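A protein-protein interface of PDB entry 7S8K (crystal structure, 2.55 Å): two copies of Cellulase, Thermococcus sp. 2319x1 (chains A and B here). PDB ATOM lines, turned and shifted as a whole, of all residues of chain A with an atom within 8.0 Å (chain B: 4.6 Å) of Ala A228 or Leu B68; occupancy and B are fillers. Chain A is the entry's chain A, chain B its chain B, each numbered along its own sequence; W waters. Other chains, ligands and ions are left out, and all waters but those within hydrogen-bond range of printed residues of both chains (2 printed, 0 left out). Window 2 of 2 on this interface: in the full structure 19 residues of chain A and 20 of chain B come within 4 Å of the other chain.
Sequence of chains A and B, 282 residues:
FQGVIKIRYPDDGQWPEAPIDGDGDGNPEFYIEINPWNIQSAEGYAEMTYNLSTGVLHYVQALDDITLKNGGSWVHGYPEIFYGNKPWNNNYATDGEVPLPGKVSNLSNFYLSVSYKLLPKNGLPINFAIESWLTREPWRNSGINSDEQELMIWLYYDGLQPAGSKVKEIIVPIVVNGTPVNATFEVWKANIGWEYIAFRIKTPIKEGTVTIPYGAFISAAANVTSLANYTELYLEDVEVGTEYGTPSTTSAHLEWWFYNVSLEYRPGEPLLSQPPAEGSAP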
ATOM      1  N   ARG A 136      32.166  -0.791  31.688  1.00  0.00           N
ATOM      2  CA  ARG A 136      32.086   0.443  32.459  1.00  0.00           C
ATOM      3  C   ARG A 136      33.196   0.572  33.499  1.00  0.00           C
ATOM      4  O   ARG A 136      33.613   1.690  33.811  1.00  0.00           O
ATOM      5  CB  ARG A 136      30.715   0.540  33.133  1.00  0.00           C
ATOM      6  CG  ARG A 136      29.552   0.651  32.154  1.00  0.00           C
ATOM      7  CD  ARG A 136      29.405   2.056  31.597  1.00  0.00           C
ATOM      8  NE  ARG A 136      28.487   2.104  30.466  1.00  0.00           N
ATOM      9  CZ  ARG A 136      28.539   3.016  29.505  1.00  0.00           C
ATOM     10  NH1 ARG A 136      29.453   3.973  29.510  1.00  0.00           N
ATOM     11  NH2 ARG A 136      27.662   2.959  28.506  1.00  0.00           N
ATOM     12  N   ASP A 147      24.433  -2.282  29.153  1.00  0.00           N
ATOM     13  CA  ASP A 147      24.944  -1.008  28.666  1.00  0.00           C
ATOM     14  C   ASP A 147      26.403  -1.088  28.234  1.00  0.00           C
ATOM     15  O   ASP A 147      27.123  -0.080  28.292  1.00  0.00           O
ATOM     16  CB  ASP A 147      24.758   0.074  29.731  1.00  0.00           C
ATOM     17  CG  ASP A 147      25.574  -0.192  30.980  1.00  0.00           C
ATOM     18  OD1 ASP A 147      25.811  -1.376  31.296  1.00  0.00           O
ATOM     19  OD2 ASP A 147      25.981   0.784  31.645  1.00  0.00           O
ATOM     20  N   GLU A 148      26.861  -2.261  27.805  1.00  0.00           N
ATOM     21  CA  GLU A 148      28.228  -2.462  27.352  1.00  0.00           C
ATOM     22  C   GLU A 148      28.201  -3.092  25.965  1.00  0.00           C
ATOM     23  O   GLU A 148      27.146  -3.488  25.462  1.00  0.00           O
ATOM     24  CB  GLU A 148      29.018  -3.319  28.352  1.00  0.00           C
ATOM     25  CG  GLU A 148      29.163  -2.644  29.713  1.00  0.00           C
ATOM     26  CD  GLU A 148      29.671  -3.575  30.795  1.00  0.00           C
ATOM     27  OE1 GLU A 148      29.520  -4.805  30.649  1.00  0.00           O
ATOM     28  OE2 GLU A 148      30.214  -3.073  31.803  1.00  0.00           O
ATOM     29  N   GLU A 195      25.294  -4.803  23.616  1.00  0.00           N
ATOM     30  CA  GLU A 195      25.323  -4.419  22.212  1.00  0.00           C
ATOM     31  C   GLU A 195      26.425  -5.197  21.508  1.00  0.00           C
ATOM     32  O   GLU A 195      27.562  -5.250  21.986  1.00  0.00           O
ATOM     33  CB  GLU A 195      25.532  -2.916  22.036  1.00  0.00           C
ATOM     34  CG  GLU A 195      25.049  -2.420  20.676  1.00  0.00           C
ATOM     35  CD  GLU A 195      25.411  -0.974  20.404  1.00  0.00           C
ATOM     36  OE1 GLU A 195      26.604  -0.624  20.533  1.00  0.00           O
ATOM     37  OE2 GLU A 195      24.505  -0.188  20.052  1.00  0.00           O
ATOM     38  N   THR A 225      26.337   2.960  17.412  1.00  0.00           N
ATOM     39  CA  THR A 225      25.922   2.425  18.700  1.00  0.00           C
ATOM     40  C   THR A 225      24.657   3.108  19.209  1.00  0.00           C
ATOM     41  O   THR A 225      24.394   4.282  18.931  1.00  0.00           O
ATOM     42  CB  THR A 225      27.046   2.576  19.734  1.00  0.00           C
ATOM     43  OG1 THR A 225      26.694   1.882  20.939  1.00  0.00           O
ATOM     44  CG2 THR A 225      27.304   4.043  20.045  1.00  0.00           C
ATOM     45  N   SER A 226      23.860   2.341  19.952  1.00  0.00           N
ATOM     46  CA  SER A 226      22.729   2.866  20.703  1.00  0.00           C
ATOM     47  C   SER A 226      23.037   2.975  22.188  1.00  0.00           C
ATOM     48  O   SER A 226      22.117   3.148  22.995  1.00  0.00           O
ATOM     49  CB  SER A 226      21.490   1.996  20.484  1.00  0.00           C
ATOM     50  OG  SER A 226      21.263   1.772  19.102  1.00  0.00           O
ATOM     51  N   LEU A 227      24.310   2.868  22.564  1.00  0.00           N
ATOM     52  CA  LEU A 227      24.727   2.981  23.952  1.00  0.00           C
ATOM     53  C   LEU A 227      24.989   4.438  24.300  1.00  0.00           C
ATOM     54  O   LEU A 227      25.622   5.170  23.534  1.00  0.00           O
ATOM     55  CB  LEU A 227      25.989   2.157  24.209  1.00  0.00           C
ATOM     56  CG  LEU A 227      25.882   0.638  24.065  1.00  0.00           C
ATOM     57  CD1 LEU A 227      27.265   0.008  24.101  1.00  0.00           C
ATOM     58  CD2 LEU A 227      24.992   0.050  25.150  1.00  0.00           C
ATOM     59  N   ALA A 228      24.492   4.854  25.457  1.00  0.00           N
ATOM     60  CA  ALA A 228      24.776   6.188  25.954  1.00  0.00           C
ATOM     61  C   ALA A 228      26.187   6.245  26.522  1.00  0.00           C
ATOM     62  O   ALA A 228      26.701   5.261  27.064  1.00  0.00           O
ATOM     63  CB  ALA A 228      23.760   6.591  27.022  1.00  0.00           C
ATOM     64  N   ASN A 229      26.818   7.412  26.379  1.00  0.00           N
ATOM     65  CA  ASN A 229      28.158   7.664  26.909  1.00  0.00           C
ATOM     66  C   ASN A 229      29.149   6.601  26.441  1.00  0.00           C
ATOM     67  O   ASN A 229      29.909   6.035  27.229  1.00  0.00           O
ATOM     68  CB  ASN A 229      28.135   7.750  28.437  1.00  0.00           C
ATOM     69  CG  ASN A 229      27.041   8.661  28.951  1.00  0.00           C
ATOM     70  OD1 ASN A 229      26.282   8.294  29.852  1.00  0.00           O
ATOM     71  ND2 ASN A 229      26.957   9.863  28.390  1.00  0.00           N
ATOM     72  N   TYR A 230      29.129   6.333  25.133  1.00  0.00           N
ATOM     73  CA  TYR A 230      29.992   5.298  24.571  1.00  0.00           C
ATOM     74  C   TYR A 230      31.464   5.597  24.832  1.00  0.00           C
ATOM     75  O   TYR A 230      32.241   4.690  25.155  1.00  0.00           O
ATOM     76  CB  TYR A 230      29.730   5.154  23.070  1.00  0.00           C
ATOM     77  CG  TYR A 230      30.562   4.077  22.406  1.00  0.00           C
ATOM     78  CD1 TYR A 230      30.205   2.739  22.506  1.00  0.00           C
ATOM     79  CD2 TYR A 230      31.707   4.398  21.685  1.00  0.00           C
ATOM     80  CE1 TYR A 230      30.965   1.751  21.906  1.00  0.00           C
ATOM     81  CE2 TYR A 230      32.473   3.415  21.080  1.00  0.00           C
ATOM     82  CZ  TYR A 230      32.097   2.093  21.193  1.00  0.00           C
ATOM     83  OH  TYR A 230      32.852   1.106  20.599  1.00  0.00           O
ATOM     84  N   THR A 231      31.864   6.865  24.715  1.00  0.00           N
ATOM     85  CA  THR A 231      33.265   7.230  24.901  1.00  0.00           C
ATOM     86  C   THR A 231      33.749   7.009  26.331  1.00  0.00           C
ATOM     87  O   THR A 231      34.963   6.980  26.561  1.00  0.00           O
ATOM     88  CB  THR A 231      33.484   8.691  24.504  1.00  0.00           C
ATOM     89  OG1 THR A 231      32.517   9.518  25.162  1.00  0.00           O
ATOM     90  CG2 THR A 231      33.340   8.855  23.004  1.00  0.00           C
ATOM     91  N   GLU A 232      32.838   6.857  27.292  1.00  0.00           N
ATOM     92  CA  GLU A 232      33.224   6.597  28.673  1.00  0.00           C
ATOM     93  C   GLU A 232      33.486   5.121  28.951  1.00  0.00           C
ATOM     94  O   GLU A 232      33.914   4.787  30.060  1.00  0.00           O
ATOM     95  CB  GLU A 232      32.148   7.121  29.630  1.00  0.00           C
ATOM     96  CG  GLU A 232      31.951   8.627  29.566  1.00  0.00           C
ATOM     97  CD  GLU A 232      30.809   9.115  30.438  1.00  0.00           C
ATOM     98  OE1 GLU A 232      30.060   8.271  30.973  1.00  0.00           O
ATOM     99  OE2 GLU A 232      30.665  10.346  30.588  1.00  0.00           O
ATOM    100  N   LEU A 233      33.245   4.239  27.983  1.00  0.00           N
ATOM    101  CA  LEU A 233      33.522   2.823  28.165  1.00  0.00           C
ATOM    102  C   LEU A 233      35.027   2.558  28.146  1.00  0.00           C
ATOM    103  O   LEU A 233      35.819   3.336  27.607  1.00  0.00           O
ATOM    104  CB  LEU A 233      32.831   1.997  27.077  1.00  0.00           C
ATOM    105  CG  LEU A 233      31.311   1.844  27.182  1.00  0.00           C
ATOM    106  CD1 LEU A 233      30.723   1.377  25.859  1.00  0.00           C
ATOM    107  CD2 LEU A 233      30.941   0.879  28.304  1.00  0.00           C
ATOM    108  N   ASN B  38      17.283   0.340  32.138  1.00  0.00           N
ATOM    109  CA  ASN B  38      17.682   0.930  30.868  1.00  0.00           C
ATOM    110  C   ASN B  38      17.465   2.435  30.817  1.00  0.00           C
ATOM    111  O   ASN B  38      17.740   3.052  29.782  1.00  0.00           O
ATOM    112  CB  ASN B  38      16.936   0.256  29.709  1.00  0.00           C
ATOM    113  CG  ASN B  38      17.658   0.412  28.383  1.00  0.00           C
ATOM    114  OD1 ASN B  38      18.883   0.537  28.336  1.00  0.00           O
ATOM    115  ND2 ASN B  38      16.895   0.404  27.292  1.00  0.00           N
ATOM    116  N   GLN B  40      18.661   5.927  31.273  1.00  0.00           N
ATOM    117  CA  GLN B  40      19.920   6.642  31.428  1.00  0.00           C
ATOM    118  C   GLN B  40      19.727   8.058  31.952  1.00  0.00           C
ATOM    119  O   GLN B  40      20.529   8.531  32.762  1.00  0.00           O
ATOM    120  CB  GLN B  40      20.669   6.676  30.094  1.00  0.00           C
ATOM    121  CG  GLN B  40      22.144   6.376  30.224  1.00  0.00           C
ATOM    122  CD  GLN B  40      22.904   7.539  30.787  1.00  0.00           C
ATOM    123  OE1 GLN B  40      22.628   8.681  30.446  1.00  0.00           O
ATOM    124  NE2 GLN B  40      23.864   7.262  31.662  1.00  0.00           N
ATOM    125  N   ILE B  66      12.729  10.547  28.105  1.00  0.00           N
ATOM    126  CA  ILE B  66      13.523   9.377  28.458  1.00  0.00           C
ATOM    127  C   ILE B  66      14.725   9.274  27.532  1.00  0.00           C
ATOM    128  O   ILE B  66      14.581   9.281  26.303  1.00  0.00           O
ATOM    129  CB  ILE B  66      12.673   8.100  28.381  1.00  0.00           C
ATOM    130  CG1 ILE B  66      11.497   8.167  29.357  1.00  0.00           C
ATOM    131  CG2 ILE B  66      13.535   6.882  28.662  1.00  0.00           C
ATOM    132  CD1 ILE B  66      11.880   8.627  30.730  1.00  0.00           C
ATOM    133  N   THR B  67      15.912   9.172  28.120  1.00  0.00           N
ATOM    134  CA  THR B  67      17.112   8.741  27.418  1.00  0.00           C
ATOM    135  C   THR B  67      17.456   7.338  27.896  1.00  0.00           C
ATOM    136  O   THR B  67      17.489   7.081  29.104  1.00  0.00           O
ATOM    137  CB  THR B  67      18.288   9.688  27.667  1.00  0.00           C
ATOM    138  OG1 THR B  67      17.924  11.017  27.277  1.00  0.00           O
ATOM    139  CG2 THR B  67      19.514   9.244  26.876  1.00  0.00           C
ATOM    140  N   LEU B  68      17.698   6.437  26.954  1.00  0.00           N
ATOM    141  CA  LEU B  68      17.924   5.037  27.275  1.00  0.00           C
ATOM    142  C   LEU B  68      19.414   4.738  27.361  1.00  0.00           C
ATOM    143  O   LEU B  68      20.239   5.396  26.721  1.00  0.00           O
ATOM    144  CB  LEU B  68      17.267   4.132  26.233  1.00  0.00           C
ATOM    145  CG  LEU B  68      15.740   4.193  26.213  1.00  0.00           C
ATOM    146  CD1 LEU B  68      15.171   3.282  25.136  1.00  0.00           C
ATOM    147  CD2 LEU B  68      15.196   3.829  27.582  1.00  0.00           C
ATOM    148  N   LYS B  69      19.751   3.736  28.174  1.00  0.00           N
ATOM    149  CA  LYS B  69      21.133   3.279  28.267  1.00  0.00           C
ATOM    150  C   LYS B  69      21.536   2.529  27.004  1.00  0.00           C
ATOM    151  O   LYS B  69      22.523   2.872  26.346  1.00  0.00           O
ATOM    152  CB  LYS B  69      21.309   2.387  29.497  1.00  0.00           C
ATOM    153  CG  LYS B  69      21.185   3.116  30.817  1.00  0.00           C
ATOM    154  CD  LYS B  69      22.009   2.447  31.898  1.00  0.00           C
ATOM    155  CE  LYS B  69      21.287   2.477  33.233  1.00  0.00           C
ATOM    156  NZ  LYS B  69      21.904   1.537  34.208  1.00  0.00           N
ATOM    157  N   ASN B  70      20.780   1.491  26.659  1.00  0.00           N
ATOM    158  CA  ASN B  70      20.971   0.729  25.429  1.00  0.00           C
ATOM    159  C   ASN B  70      19.665   0.814  24.647  1.00  0.00           C
ATOM    160  O   ASN B  70      18.678   0.164  25.004  1.00  0.00           O
ATOM    161  CB  ASN B  70      21.356  -0.718  25.728  1.00  0.00           C
ATOM    162  CG  ASN B  70      21.823  -1.463  24.494  1.00  0.00           C
ATOM    163  OD1 ASN B  70      21.791  -0.931  23.384  1.00  0.00           O
ATOM    164  ND2 ASN B  70      22.257  -2.703  24.680  1.00  0.00           N
ATOM    165  N   GLY B  71      19.624   1.657  23.636  1.00  0.00           N
ATOM    166  CA  GLY B  71      18.446   1.781  22.826  1.00  0.00           C
ATOM    167  C   GLY B  71      18.083   0.461  22.229  1.00  0.00           C
ATOM    168  O   GLY B  71      16.976   0.262  21.851  1.00  0.00           O
ATOM    169  N   TRP B  74      15.527  -2.155  23.966  1.00  0.00           N
ATOM    170  CA  TRP B  74      14.101  -1.864  23.833  1.00  0.00           C
ATOM    171  C   TRP B  74      13.326  -1.358  25.041  1.00  0.00           C
ATOM    172  O   TRP B  74      12.927  -0.238  25.073  1.00  0.00           O
ATOM    173  CB  TRP B  74      13.377  -3.022  23.162  1.00  0.00           C
ATOM    174  CG  TRP B  74      12.261  -2.655  22.371  1.00  0.00           C
ATOM    175  CD1 TRP B  74      11.018  -2.581  22.771  1.00  0.00           C
ATOM    176  CD2 TRP B  74      12.275  -2.333  21.006  1.00  0.00           C
ATOM    177  NE1 TRP B  74      10.219  -2.216  21.761  1.00  0.00           N
ATOM    178  CE2 TRP B  74      10.975  -2.065  20.644  1.00  0.00           C
ATOM    179  CE3 TRP B  74      13.274  -2.238  20.045  1.00  0.00           C
ATOM    180  CZ2 TRP B  74      10.628  -1.693  19.372  1.00  0.00           C
ATOM    181  CZ3 TRP B  74      12.935  -1.881  18.805  1.00  0.00           C
ATOM    182  CH2 TRP B  74      11.626  -1.605  18.470  1.00  0.00           C
ATOM    183  N   HIS B  76      12.341  -0.053  28.830  1.00  0.00           N
ATOM    184  CA  HIS B  76      12.941   0.971  29.679  1.00  0.00           C
ATOM    185  C   HIS B  76      13.326   0.423  31.050  1.00  0.00           C
ATOM    186  O   HIS B  76      14.424   0.694  31.546  1.00  0.00           O
ATOM    187  CB  HIS B  76      11.980   2.154  29.843  1.00  0.00           C
ATOM    188  CG  HIS B  76      11.761   2.942  28.590  1.00  0.00           C
ATOM    189  ND1 HIS B  76      11.199   4.199  28.594  1.00  0.00           N
ATOM    190  CD2 HIS B  76      12.026   2.652  27.294  1.00  0.00           C
ATOM    191  CE1 HIS B  76      11.128   4.651  27.354  1.00  0.00           C
ATOM    192  NE2 HIS B  76      11.624   3.732  26.547  1.00  0.00           N
ATOM    193  N   THR B 246       9.646   1.714  24.762  1.00  0.00           N
ATOM    194  CA  THR B 246      10.306   1.351  23.519  1.00  0.00           C
ATOM    195  C   THR B 246      11.351   2.408  23.203  1.00  0.00           C
ATOM    196  O   THR B 246      11.338   3.495  23.790  1.00  0.00           O
ATOM    197  CB  THR B 246       9.299   1.244  22.362  1.00  0.00           C
ATOM    198  OG1 THR B 246       8.798   2.546  22.034  1.00  0.00           O
ATOM    199  CG2 THR B 246       8.145   0.321  22.726  1.00  0.00           C
ATOM    200  N   PRO B 247      12.287   2.116  22.292  1.00  0.00           N
ATOM    201  CA  PRO B 247      13.278   3.140  21.915  1.00  0.00           C
ATOM    202  C   PRO B 247      12.660   4.439  21.429  1.00  0.00           C
ATOM    203  O   PRO B 247      13.262   5.505  21.610  1.00  0.00           O
ATOM    204  CB  PRO B 247      14.083   2.451  20.807  1.00  0.00           C
ATOM    205  CG  PRO B 247      13.963   1.005  21.110  1.00  0.00           C
ATOM    206  CD  PRO B 247      12.601   0.805  21.698  1.00  0.00           C
HETATM  207  O   HOH W   1      21.129   5.322  24.090  1.00  0.00           O
HETATM  208  O   HOH W   2      26.849   5.494  31.435  1.00  0.00           O
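The backbone NH (N) of Gly B71 lies within hydrogen-bond range of the backbone carbonyl oxygen (O) of Ser A226 (3.0 Å).
The backbone NH of Ala A228 sits at hydrogen-bond distance from the backbone carbonyl oxygen of Lys B69 (2.9 Å).
The side-chain amide nitrogen of Gln B40 sits at hydrogen-bond distance from the side-chain amide oxygen of Asn A229 (3.2 Å).
The backbone carbonyl oxygen of Lys B69 sits close to the backbone carbonyl oxygen of Ser A226, at 3.4 Å.
NH2 of Arg A136 sits at hydrogen-bond distance from O of Ala A228, 2.9 Å away.
The backbone NH (N) of Glu A195 sits at hydrogen-bond distance from the backbone carbonyl oxygen (O) of Glu A148, at 2.9 Å.
The side-chain carboxylate (OE1) of Glu A195 lies within hydrogen-bond range of the side-chain hydroxyl (OG1) of Thr A225 (2.5 Å).
The backbone NH (N) of Leu A227 lies within hydrogen-bond range of the side-chain hydroxyl (OG1) of Thr A225 (3.0 Å).
The backbone carbonyl oxygen of Asn B38 is in hydrogen-bond range of the backbone NH of Lys B69, 2.7 Å away.
The backbone NH (N) of Gln B40 sits at hydrogen-bond distance from the backbone carbonyl oxygen (O) of Thr B67, at 2.7 Å.
Glu A195 touches Asn B70.
O of Ser A226 touches CA of Asn B70, at 3.6 Å.
CA of Leu A227 touches O of Lys B69, 3.3 Å away.
CD2 of Leu A227 touches CG of Asn B70, at 3.6 Å.
Ala A228 touches Gln B40 (CB to CG, 3.6 Å).
O of Leu B68 touches CB of Ala A228, 3.7 Å away.
Of the printed residues of chain B, Ser A226 touches Lys B69, Asn B70 and Gly B71.
Of chain B, only Gln B40 (3.6 Å), Leu B68 (3.7 Å) and Lys B69 (2.9 Å) come within 4 Å of Ala A228.
Printed residues of chain A within 4 Å of Leu B68: Ala A228 (3.7 Å).
Of the printed residues of chain A, Lys B69 touches Ser A226 (3.4 Å), Leu A227 (3.3 Å) and Ala A228 (2.9 Å).
Of the printed residues of chain A, Asn B70 touches Glu A195, Ser A226 and Leu A227.
The nearest residue of chain A that does not touch Leu B68 is Ser A226 (4.7 Å).
The nearest printed residue of chain B that does not touch Ser A226 is Leu B68 (4.7 Å).
Printed residues of chain A that touch a printed residue of chain B: Glu A195, Ser A226, Leu A227, Ala A228 and Asn A229.
Among the printed residues, 10 pairs touch across the chains.
No position is printed for both chains.
Of the 10 pairs that touch across the chains among the printed residues, none has its exchanged pair printed and touching as well.
Water W1 bridges O of Ser A226 (2.6 Å) and O of Leu B68 (2.8 Å).
Water W2 bridges OD1 of Asn A229 (3.3 Å) and NE2 of Gln B40 (3.5 Å).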
